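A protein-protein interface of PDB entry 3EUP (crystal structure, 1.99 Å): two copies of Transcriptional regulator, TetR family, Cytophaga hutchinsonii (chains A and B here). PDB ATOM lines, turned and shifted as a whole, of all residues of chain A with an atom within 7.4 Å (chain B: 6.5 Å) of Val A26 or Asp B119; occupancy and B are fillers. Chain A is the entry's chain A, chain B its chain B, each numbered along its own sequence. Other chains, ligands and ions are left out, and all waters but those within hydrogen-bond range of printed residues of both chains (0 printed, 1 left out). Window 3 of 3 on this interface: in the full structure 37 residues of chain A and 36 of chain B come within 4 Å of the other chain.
Hydrophobic or aromatic side chains of chain A within 4 Å of the printed part of chain B: Val A26. Along chain A the printed residues that touch a printed residue of chain B span positions 26 to 180. Among the printed residues, Asp or Glu carboxylates within 4 Å of a Lys or Arg side-chain nitrogen of the other chain: Arg A177 with Asp B118 (3.7 Å) and Arg A177 with Asp B119 (2.3 Å).
No position is printed for both chains.
Val A26 touches just these residues of chain B: Asp B119 (3.7 Å) and Thr B120 (3.6 Å). Of the printed residues of chain B, Gly A106 touches Asp B119. Of the printed residues of chain A, Thr B120 touches Val A26. Printed residues of chain B within 4 Å of Asn A112: Ile B115 (3.3 Å). Printed residues of chain A within 4 Å of Ile B115: Asn A112 (3.3 Å). Printed residues of chain A within 4 Å of Asp B118: Arg A177. The nearest residue of chain B that does not touch Val A26 is Glu B116 (4.5 Å). The nearest residue of chain A that does not touch Asp B119 is Gly A107 (5.0 Å).
The side-chain carboxylate (OD1) of Asp B119 is in salt-bridge range of the guanidinium group (NH1) of Arg A177 (3.4 Å). NH1 of Arg A177 is in salt-bridge range of OD2 of Asp B118.
The backbone carbonyl oxygen (O) of Gly A106 lies within hydrogen-bond range of the side-chain amide nitrogen (ND2) of Asn A112 (2.9 Å). OD1 of Asn A25 lies within hydrogen-bond range of ND2 of Asn A112 (2.9 Å). The backbone carbonyl oxygen (O) of Gly A106 sits close to the guanidinium group (NH1) of Arg A177 (3.1 Å). The side-chain hydroxyl (OG1) of Thr B120 lies within hydrogen-bond range of the backbone carbonyl oxygen (O) of Glu B116.
Among the printed residues, merely in contact across the chains: Asn A112 with Ile B115 (3.3 Å), Arg A177 with Arg B125 (3.5 Å), Gly A106 with Asp B119 (3.5 Å), Val A26 with Thr B120 (3.6 Å), Lys A180 with Arg B125 (3.6 Å), Val A26 with Asp B119 (3.7 Å) and Arg A177 with Thr B114 (3.8 Å).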
ATOM      1  N   THR A  20      24.486  -2.107 -12.151  1.00  0.00           N
ATOM      2  CA  THR A  20      23.385  -2.447 -11.277  1.00  0.00           C
ATOM      3  C   THR A  20      23.189  -1.479 -10.139  1.00  0.00           C
ATOM      4  O   THR A  20      22.139  -1.515  -9.527  1.00  0.00           O
ATOM      5  CB  THR A  20      23.511  -3.853 -10.667  1.00  0.00           C
ATOM      6  OG1 THR A  20      24.659  -3.904  -9.802  1.00  0.00           O
ATOM      7  CG2 THR A  20      23.619  -4.917 -11.800  1.00  0.00           C
ATOM      8  N   ALA A  21      24.187  -0.642  -9.854  1.00  0.00           N
ATOM      9  CA  ALA A  21      24.097   0.332  -8.746  1.00  0.00           C
ATOM     10  C   ALA A  21      22.887   1.290  -8.854  1.00  0.00           C
ATOM     11  O   ALA A  21      22.275   1.634  -7.823  1.00  0.00           O
ATOM     12  CB  ALA A  21      25.401   1.129  -8.601  1.00  0.00           C
ATOM     13  N   PRO A  22      22.539   1.745 -10.064  1.00  0.00           N
ATOM     14  CA  PRO A  22      21.332   2.595 -10.198  1.00  0.00           C
ATOM     15  C   PRO A  22      20.043   1.828  -9.921  1.00  0.00           C
ATOM     16  O   PRO A  22      19.065   2.407  -9.433  1.00  0.00           O
ATOM     17  CB  PRO A  22      21.369   3.021 -11.675  1.00  0.00           C
ATOM     18  CG  PRO A  22      22.769   2.844 -12.082  1.00  0.00           C
ATOM     19  CD  PRO A  22      23.297   1.692 -11.320  1.00  0.00           C
ATOM     20  N   VAL A  23      20.023   0.530 -10.219  1.00  0.00           N
ATOM     21  CA  VAL A  23      18.850  -0.278  -9.933  1.00  0.00           C
ATOM     22  C   VAL A  23      18.762  -0.478  -8.418  1.00  0.00           C
ATOM     23  O   VAL A  23      17.671  -0.353  -7.837  1.00  0.00           O
ATOM     24  CB  VAL A  23      18.879  -1.679 -10.599  1.00  0.00           C
ATOM     25  CG1 VAL A  23      17.577  -2.378 -10.368  1.00  0.00           C
ATOM     26  CG2 VAL A  23      19.163  -1.568 -12.128  1.00  0.00           C
ATOM     27  N   PHE A  24      19.857  -0.838  -7.749  1.00  0.00           N
ATOM     28  CA  PHE A  24      19.729  -1.007  -6.291  1.00  0.00           C
ATOM     29  C   PHE A  24      19.326   0.309  -5.631  1.00  0.00           C
ATOM     30  O   PHE A  24      18.536   0.316  -4.696  1.00  0.00           O
ATOM     31  CB  PHE A  24      20.992  -1.531  -5.631  1.00  0.00           C
ATOM     32  CG  PHE A  24      21.213  -2.987  -5.840  1.00  0.00           C
ATOM     33  CD1 PHE A  24      20.400  -3.937  -5.204  1.00  0.00           C
ATOM     34  CD2 PHE A  24      22.185  -3.417  -6.715  1.00  0.00           C
ATOM     35  CE1 PHE A  24      20.599  -5.317  -5.409  1.00  0.00           C
ATOM     36  CE2 PHE A  24      22.390  -4.796  -6.952  1.00  0.00           C
ATOM     37  CZ  PHE A  24      21.604  -5.736  -6.293  1.00  0.00           C
ATOM     38  N   ASN A  25      19.879   1.419  -6.096  1.00  0.00           N
ATOM     39  CA  ASN A  25      19.623   2.721  -5.471  1.00  0.00           C
ATOM     40  C   ASN A  25      18.157   3.134  -5.575  1.00  0.00           C
ATOM     41  O   ASN A  25      17.668   3.834  -4.699  1.00  0.00           O
ATOM     42  CB  ASN A  25      20.528   3.816  -6.024  1.00  0.00           C
ATOM     43  CG  ASN A  25      20.617   5.017  -5.115  1.00  0.00           C
ATOM     44  OD1 ASN A  25      20.673   4.891  -3.884  1.00  0.00           O
ATOM     45  ND2 ASN A  25      20.619   6.191  -5.707  1.00  0.00           N
ATOM     46  N   VAL A  26      17.470   2.647  -6.598  1.00  0.00           N
ATOM     47  CA  VAL A  26      16.060   2.967  -6.870  1.00  0.00           C
ATOM     48  C   VAL A  26      15.093   1.940  -6.284  1.00  0.00           C
ATOM     49  O   VAL A  26      14.145   2.296  -5.580  1.00  0.00           O
ATOM     50  CB  VAL A  26      15.838   3.090  -8.399  1.00  0.00           C
ATOM     51  CG1 VAL A  26      14.311   3.056  -8.779  1.00  0.00           C
ATOM     52  CG2 VAL A  26      16.461   4.366  -8.877  1.00  0.00           C
ATOM     53  N   LYS A  27      15.365   0.665  -6.526  1.00  0.00           N
ATOM     54  CA  LYS A  27      14.452  -0.416  -6.153  1.00  0.00           C
ATOM     55  C   LYS A  27      14.761  -1.052  -4.798  1.00  0.00           C
ATOM     56  O   LYS A  27      13.917  -1.764  -4.231  1.00  0.00           O
ATOM     57  CB  LYS A  27      14.479  -1.503  -7.221  1.00  0.00           C
ATOM     58  CG  LYS A  27      14.031  -1.028  -8.585  1.00  0.00           C
ATOM     59  CD  LYS A  27      13.788  -2.240  -9.506  1.00  0.00           C
ATOM     60  CE  LYS A  27      12.859  -1.915 -10.666  1.00  0.00           C
ATOM     61  NZ  LYS A  27      12.596  -3.127 -11.492  1.00  0.00           N
ATOM     62  N   GLY A  28      15.967  -0.831  -4.277  1.00  0.00           N
ATOM     63  CA  GLY A  28      16.331  -1.428  -3.006  1.00  0.00           C
ATOM     64  C   GLY A  28      16.721  -2.886  -3.173  1.00  0.00           C
ATOM     65  O   GLY A  28      16.622  -3.436  -4.240  1.00  0.00           O
ATOM     66  N   LEU A  29      17.228  -3.487  -2.119  1.00  0.00           N
ATOM     67  CA  LEU A  29      17.639  -4.889  -2.185  1.00  0.00           C
ATOM     68  C   LEU A  29      16.394  -5.774  -2.402  1.00  0.00           C
ATOM     69  O   LEU A  29      16.389  -6.627  -3.282  1.00  0.00           O
ATOM     70  CB  LEU A  29      18.417  -5.257  -0.924  1.00  0.00           C
ATOM     71  CG  LEU A  29      18.732  -6.738  -0.689  1.00  0.00           C
ATOM     72  CD1 LEU A  29      19.737  -7.294  -1.731  1.00  0.00           C
ATOM     73  CD2 LEU A  29      19.191  -6.980   0.798  1.00  0.00           C
ATOM     74  N   GLY A  31      13.461  -4.963  -3.731  1.00  0.00           N
ATOM     75  CA  GLY A  31      12.786  -4.740  -4.995  1.00  0.00           C
ATOM     76  C   GLY A  31      13.608  -5.114  -6.231  1.00  0.00           C
ATOM     77  O   GLY A  31      13.113  -5.068  -7.363  1.00  0.00           O
ATOM     78  N   THR A  32      14.874  -5.468  -6.028  1.00  0.00           N
ATOM     79  CA  THR A  32      15.743  -5.762  -7.157  1.00  0.00           C
ATOM     80  C   THR A  32      15.768  -7.254  -7.346  1.00  0.00           C
ATOM     81  O   THR A  32      16.164  -7.975  -6.440  1.00  0.00           O
ATOM     82  CB  THR A  32      17.167  -5.191  -6.927  1.00  0.00           C
ATOM     83  OG1 THR A  32      17.077  -3.751  -6.877  1.00  0.00           O
ATOM     84  CG2 THR A  32      18.119  -5.592  -8.066  1.00  0.00           C
ATOM     85  N   ASN A  66      27.957   3.732  -5.077  1.00  0.00           N
ATOM     86  CA  ASN A  66      27.035   4.877  -5.018  1.00  0.00           C
ATOM     87  C   ASN A  66      27.459   5.978  -4.064  1.00  0.00           C
ATOM     88  O   ASN A  66      27.532   7.168  -4.440  1.00  0.00           O
ATOM     89  CB  ASN A  66      25.618   4.388  -4.666  1.00  0.00           C
ATOM     90  CG  ASN A  66      24.897   3.811  -5.870  1.00  0.00           C
ATOM     91  OD1 ASN A  66      24.030   2.941  -5.738  1.00  0.00           O
ATOM     92  ND2 ASN A  66      25.272   4.269  -7.049  1.00  0.00           N
ATOM     93  N   PRO A 104      23.991   9.926  -7.710  1.00  0.00           N
ATOM     94  CA  PRO A 104      23.600   8.707  -8.409  1.00  0.00           C
ATOM     95  C   PRO A 104      22.122   8.758  -8.804  1.00  0.00           C
ATOM     96  O   PRO A 104      21.318   9.464  -8.182  1.00  0.00           O
ATOM     97  CB  PRO A 104      23.815   7.601  -7.372  1.00  0.00           C
ATOM     98  CG  PRO A 104      24.632   8.205  -6.285  1.00  0.00           C
ATOM     99  CD  PRO A 104      24.406   9.681  -6.322  1.00  0.00           C
ATOM    100  N   VAL A 105      21.785   8.018  -9.854  1.00  0.00           N
ATOM    101  CA  VAL A 105      20.378   7.791 -10.200  1.00  0.00           C
ATOM    102  C   VAL A 105      19.628   7.247  -8.980  1.00  0.00           C
ATOM    103  O   VAL A 105      20.090   6.310  -8.360  1.00  0.00           O
ATOM    104  CB  VAL A 105      20.242   6.777 -11.341  1.00  0.00           C
ATOM    105  CG1 VAL A 105      18.766   6.353 -11.523  1.00  0.00           C
ATOM    106  CG2 VAL A 105      20.797   7.384 -12.641  1.00  0.00           C
ATOM    107  N   GLY A 106      18.487   7.840  -8.646  1.00  0.00           N
ATOM    108  CA  GLY A 106      17.746   7.460  -7.425  1.00  0.00           C
ATOM    109  C   GLY A 106      18.056   8.265  -6.177  1.00  0.00           C
ATOM    110  O   GLY A 106      17.401   8.076  -5.148  1.00  0.00           O
ATOM    111  N   GLY A 107      19.054   9.148  -6.231  1.00  0.00           N
ATOM    112  CA  GLY A 107      19.296  10.098  -5.146  1.00  0.00           C
ATOM    113  C   GLY A 107      20.328   9.587  -4.168  1.00  0.00           C
ATOM    114  O   GLY A 107      21.270   8.881  -4.572  1.00  0.00           O
ATOM    115  N   ASN A 112      18.685   6.274   1.099  1.00  0.00           N
ATOM    116  CA  ASN A 112      17.945   5.180   0.538  1.00  0.00           C
ATOM    117  C   ASN A 112      18.270   3.871   1.201  1.00  0.00           C
ATOM    118  O   ASN A 112      17.369   3.006   1.416  1.00  0.00           O
ATOM    119  CB  ASN A 112      18.194   5.040  -0.971  1.00  0.00           C
ATOM    120  CG  ASN A 112      17.817   6.287  -1.745  1.00  0.00           C
ATOM    121  OD1 ASN A 112      17.181   7.218  -1.208  1.00  0.00           O
ATOM    122  ND2 ASN A 112      18.282   6.358  -2.997  1.00  0.00           N
ATOM    123  N   ARG A 177      12.491  14.939  -2.850  1.00  0.00           N
ATOM    124  CA  ARG A 177      12.026  13.633  -3.367  1.00  0.00           C
ATOM    125  C   ARG A 177      10.521  13.383  -3.182  1.00  0.00           C
ATOM    126  O   ARG A 177       9.868  12.826  -4.078  1.00  0.00           O
ATOM    127  CB  ARG A 177      12.954  12.491  -2.930  1.00  0.00           C
ATOM    128  CG  ARG A 177      14.510  12.739  -3.614  1.00  0.00           C
ATOM    129  CD  ARG A 177      15.127  11.514  -4.362  1.00  0.00           C
ATOM    130  NE  ARG A 177      15.879  11.921  -5.564  1.00  0.00           N
ATOM    131  CZ  ARG A 177      16.034  11.196  -6.657  1.00  0.00           C
ATOM    132  NH1 ARG A 177      15.531   9.997  -6.776  1.00  0.00           N
ATOM    133  NH2 ARG A 177      16.723  11.678  -7.669  1.00  0.00           N
ATOM    134  N   LYS A 180       8.897  16.774  -5.401  1.00  0.00           N
ATOM    135  CA  LYS A 180       9.422  17.037  -6.766  1.00  0.00           C
ATOM    136  C   LYS A 180       9.632  18.531  -7.046  1.00  0.00           C
ATOM    137  O   LYS A 180       9.665  18.963  -8.213  1.00  0.00           O
ATOM    138  CB  LYS A 180       8.495  16.465  -7.869  1.00  0.00           C
ATOM    139  CG  LYS A 180       8.349  14.944  -7.846  1.00  0.00           C
ATOM    140  CD  LYS A 180       7.294  14.470  -8.862  1.00  0.00           C
ATOM    141  CE  LYS A 180       7.873  13.877 -10.125  1.00  0.00           C
ATOM    142  NZ  LYS A 180       6.761  13.517 -11.101  1.00  0.00           N
ATOM    143  N   THR B 114       8.646   7.855   1.226  1.00  0.00           N
ATOM    144  CA  THR B 114       9.233   8.700   0.204  1.00  0.00           C
ATOM    145  C   THR B 114      10.392   7.972  -0.489  1.00  0.00           C
ATOM    146  O   THR B 114      10.457   7.927  -1.721  1.00  0.00           O
ATOM    147  CB  THR B 114       9.745  10.021   0.777  1.00  0.00           C
ATOM    148  OG1 THR B 114       8.633  10.744   1.322  1.00  0.00           O
ATOM    149  CG2 THR B 114      10.430  10.865  -0.332  1.00  0.00           C
ATOM    150  N   ILE B 115      11.276   7.382   0.311  1.00  0.00           N
ATOM    151  CA  ILE B 115      12.468   6.742  -0.214  1.00  0.00           C
ATOM    152  C   ILE B 115      12.058   5.609  -1.116  1.00  0.00           C
ATOM    153  O   ILE B 115      12.686   5.408  -2.116  1.00  0.00           O
ATOM    154  CB  ILE B 115      13.394   6.270   0.902  1.00  0.00           C
ATOM    155  CG1 ILE B 115      13.768   7.424   1.786  1.00  0.00           C
ATOM    156  CG2 ILE B 115      14.711   5.673   0.354  1.00  0.00           C
ATOM    157  CD1 ILE B 115      14.471   8.586   1.111  1.00  0.00           C
ATOM    158  N   GLU B 116      10.990   4.865  -0.810  1.00  0.00           N
ATOM    159  CA  GLU B 116      10.658   3.748  -1.665  1.00  0.00           C
ATOM    160  C   GLU B 116       9.899   4.240  -2.894  1.00  0.00           C
ATOM    161  O   GLU B 116      10.221   3.881  -4.034  1.00  0.00           O
ATOM    162  CB  GLU B 116       9.869   2.701  -0.918  1.00  0.00           C
ATOM    163  CG  GLU B 116       9.619   1.484  -1.834  1.00  0.00           C
ATOM    164  CD  GLU B 116       8.925   0.334  -1.156  1.00  0.00           C
ATOM    165  OE1 GLU B 116       8.194   0.588  -0.131  1.00  0.00           O
ATOM    166  OE2 GLU B 116       9.113  -0.812  -1.662  1.00  0.00           O
ATOM    167  N   ALA B 117       8.938   5.124  -2.678  1.00  0.00           N
ATOM    168  CA  ALA B 117       8.006   5.466  -3.763  1.00  0.00           C
ATOM    169  C   ALA B 117       8.541   6.512  -4.728  1.00  0.00           C
ATOM    170  O   ALA B 117       8.027   6.644  -5.862  1.00  0.00           O
ATOM    171  CB  ALA B 117       6.644   5.947  -3.163  1.00  0.00           C
ATOM    172  N   ASP B 118       9.535   7.309  -4.300  1.00  0.00           N
ATOM    173  CA  ASP B 118       9.922   8.480  -5.043  1.00  0.00           C
ATOM    174  C   ASP B 118      10.229   8.111  -6.511  1.00  0.00           C
ATOM    175  O   ASP B 118       9.736   8.792  -7.396  1.00  0.00           O
ATOM    176  CB  ASP B 118      11.005   9.364  -4.358  1.00  0.00           C
ATOM    177  CG  ASP B 118      12.342   8.655  -4.169  1.00  0.00           C
ATOM    178  OD1 ASP B 118      12.387   7.444  -4.308  1.00  0.00           O
ATOM    179  OD2 ASP B 118      13.361   9.315  -3.874  1.00  0.00           O
ATOM    180  N   ASP B 119      10.930   6.998  -6.761  1.00  0.00           N
ATOM    181  CA  ASP B 119      11.266   6.592  -8.128  1.00  0.00           C
ATOM    182  C   ASP B 119      10.601   5.266  -8.564  1.00  0.00           C
ATOM    183  O   ASP B 119      11.018   4.655  -9.529  1.00  0.00           O
ATOM    184  CB  ASP B 119      12.777   6.571  -8.295  1.00  0.00           C
ATOM    185  CG  ASP B 119      13.405   7.978  -8.103  1.00  0.00           C
ATOM    186  OD1 ASP B 119      13.022   8.918  -8.818  1.00  0.00           O
ATOM    187  OD2 ASP B 119      14.276   8.163  -7.225  1.00  0.00           O
ATOM    188  N   THR B 120       9.554   4.841  -7.866  1.00  0.00           N
ATOM    189  CA  THR B 120       8.891   3.584  -8.178  1.00  0.00           C
ATOM    190  C   THR B 120       7.350   3.655  -8.281  1.00  0.00           C
ATOM    191  O   THR B 120       6.766   2.781  -8.924  1.00  0.00           O
ATOM    192  CB  THR B 120       9.272   2.457  -7.175  1.00  0.00           C
ATOM    193  OG1 THR B 120       8.726   2.737  -5.888  1.00  0.00           O
ATOM    194  CG2 THR B 120      10.807   2.322  -7.026  1.00  0.00           C
ATOM    195  N   HIS B 121       6.694   4.620  -7.638  1.00  0.00           N
ATOM    196  CA  HIS B 121       5.242   4.515  -7.333  1.00  0.00           C
ATOM    197  C   HIS B 121       4.662   5.907  -7.201  1.00  0.00           C
ATOM    198  O   HIS B 121       4.636   6.497  -6.123  1.00  0.00           O
ATOM    199  CB  HIS B 121       4.993   3.694  -6.031  1.00  0.00           C
ATOM    200  CG  HIS B 121       3.554   3.323  -5.769  1.00  0.00           C
ATOM    201  ND1 HIS B 121       3.134   2.768  -4.570  1.00  0.00           N
ATOM    202  CD2 HIS B 121       2.434   3.464  -6.523  1.00  0.00           C
ATOM    203  CE1 HIS B 121       1.832   2.549  -4.621  1.00  0.00           C
ATOM    204  NE2 HIS B 121       1.384   2.974  -5.792  1.00  0.00           N
ATOM    205  N   ARG B 125       4.056   8.354  -3.988  1.00  0.00           N
ATOM    206  CA  ARG B 125       4.929   9.547  -3.929  1.00  0.00           C
ATOM    207  C   ARG B 125       4.041  10.782  -3.702  1.00  0.00           C
ATOM    208  O   ARG B 125       4.337  11.611  -2.847  1.00  0.00           O
ATOM    209  CB  ARG B 125       5.762   9.692  -5.213  1.00  0.00           C
ATOM    210  CG  ARG B 125       6.974  10.606  -5.110  1.00  0.00           C
ATOM    211  CD  ARG B 125       6.665  12.069  -5.265  1.00  0.00           C
ATOM    212  NE  ARG B 125       5.701  12.378  -6.322  1.00  0.00           N
ATOM    213  CZ  ARG B 125       4.911  13.445  -6.305  1.00  0.00           C
ATOM    214  NH1 ARG B 125       4.968  14.323  -5.299  1.00  0.00           N
ATOM    215  NH2 ARG B 125       4.042  13.634  -7.293  1.00  0.00           N
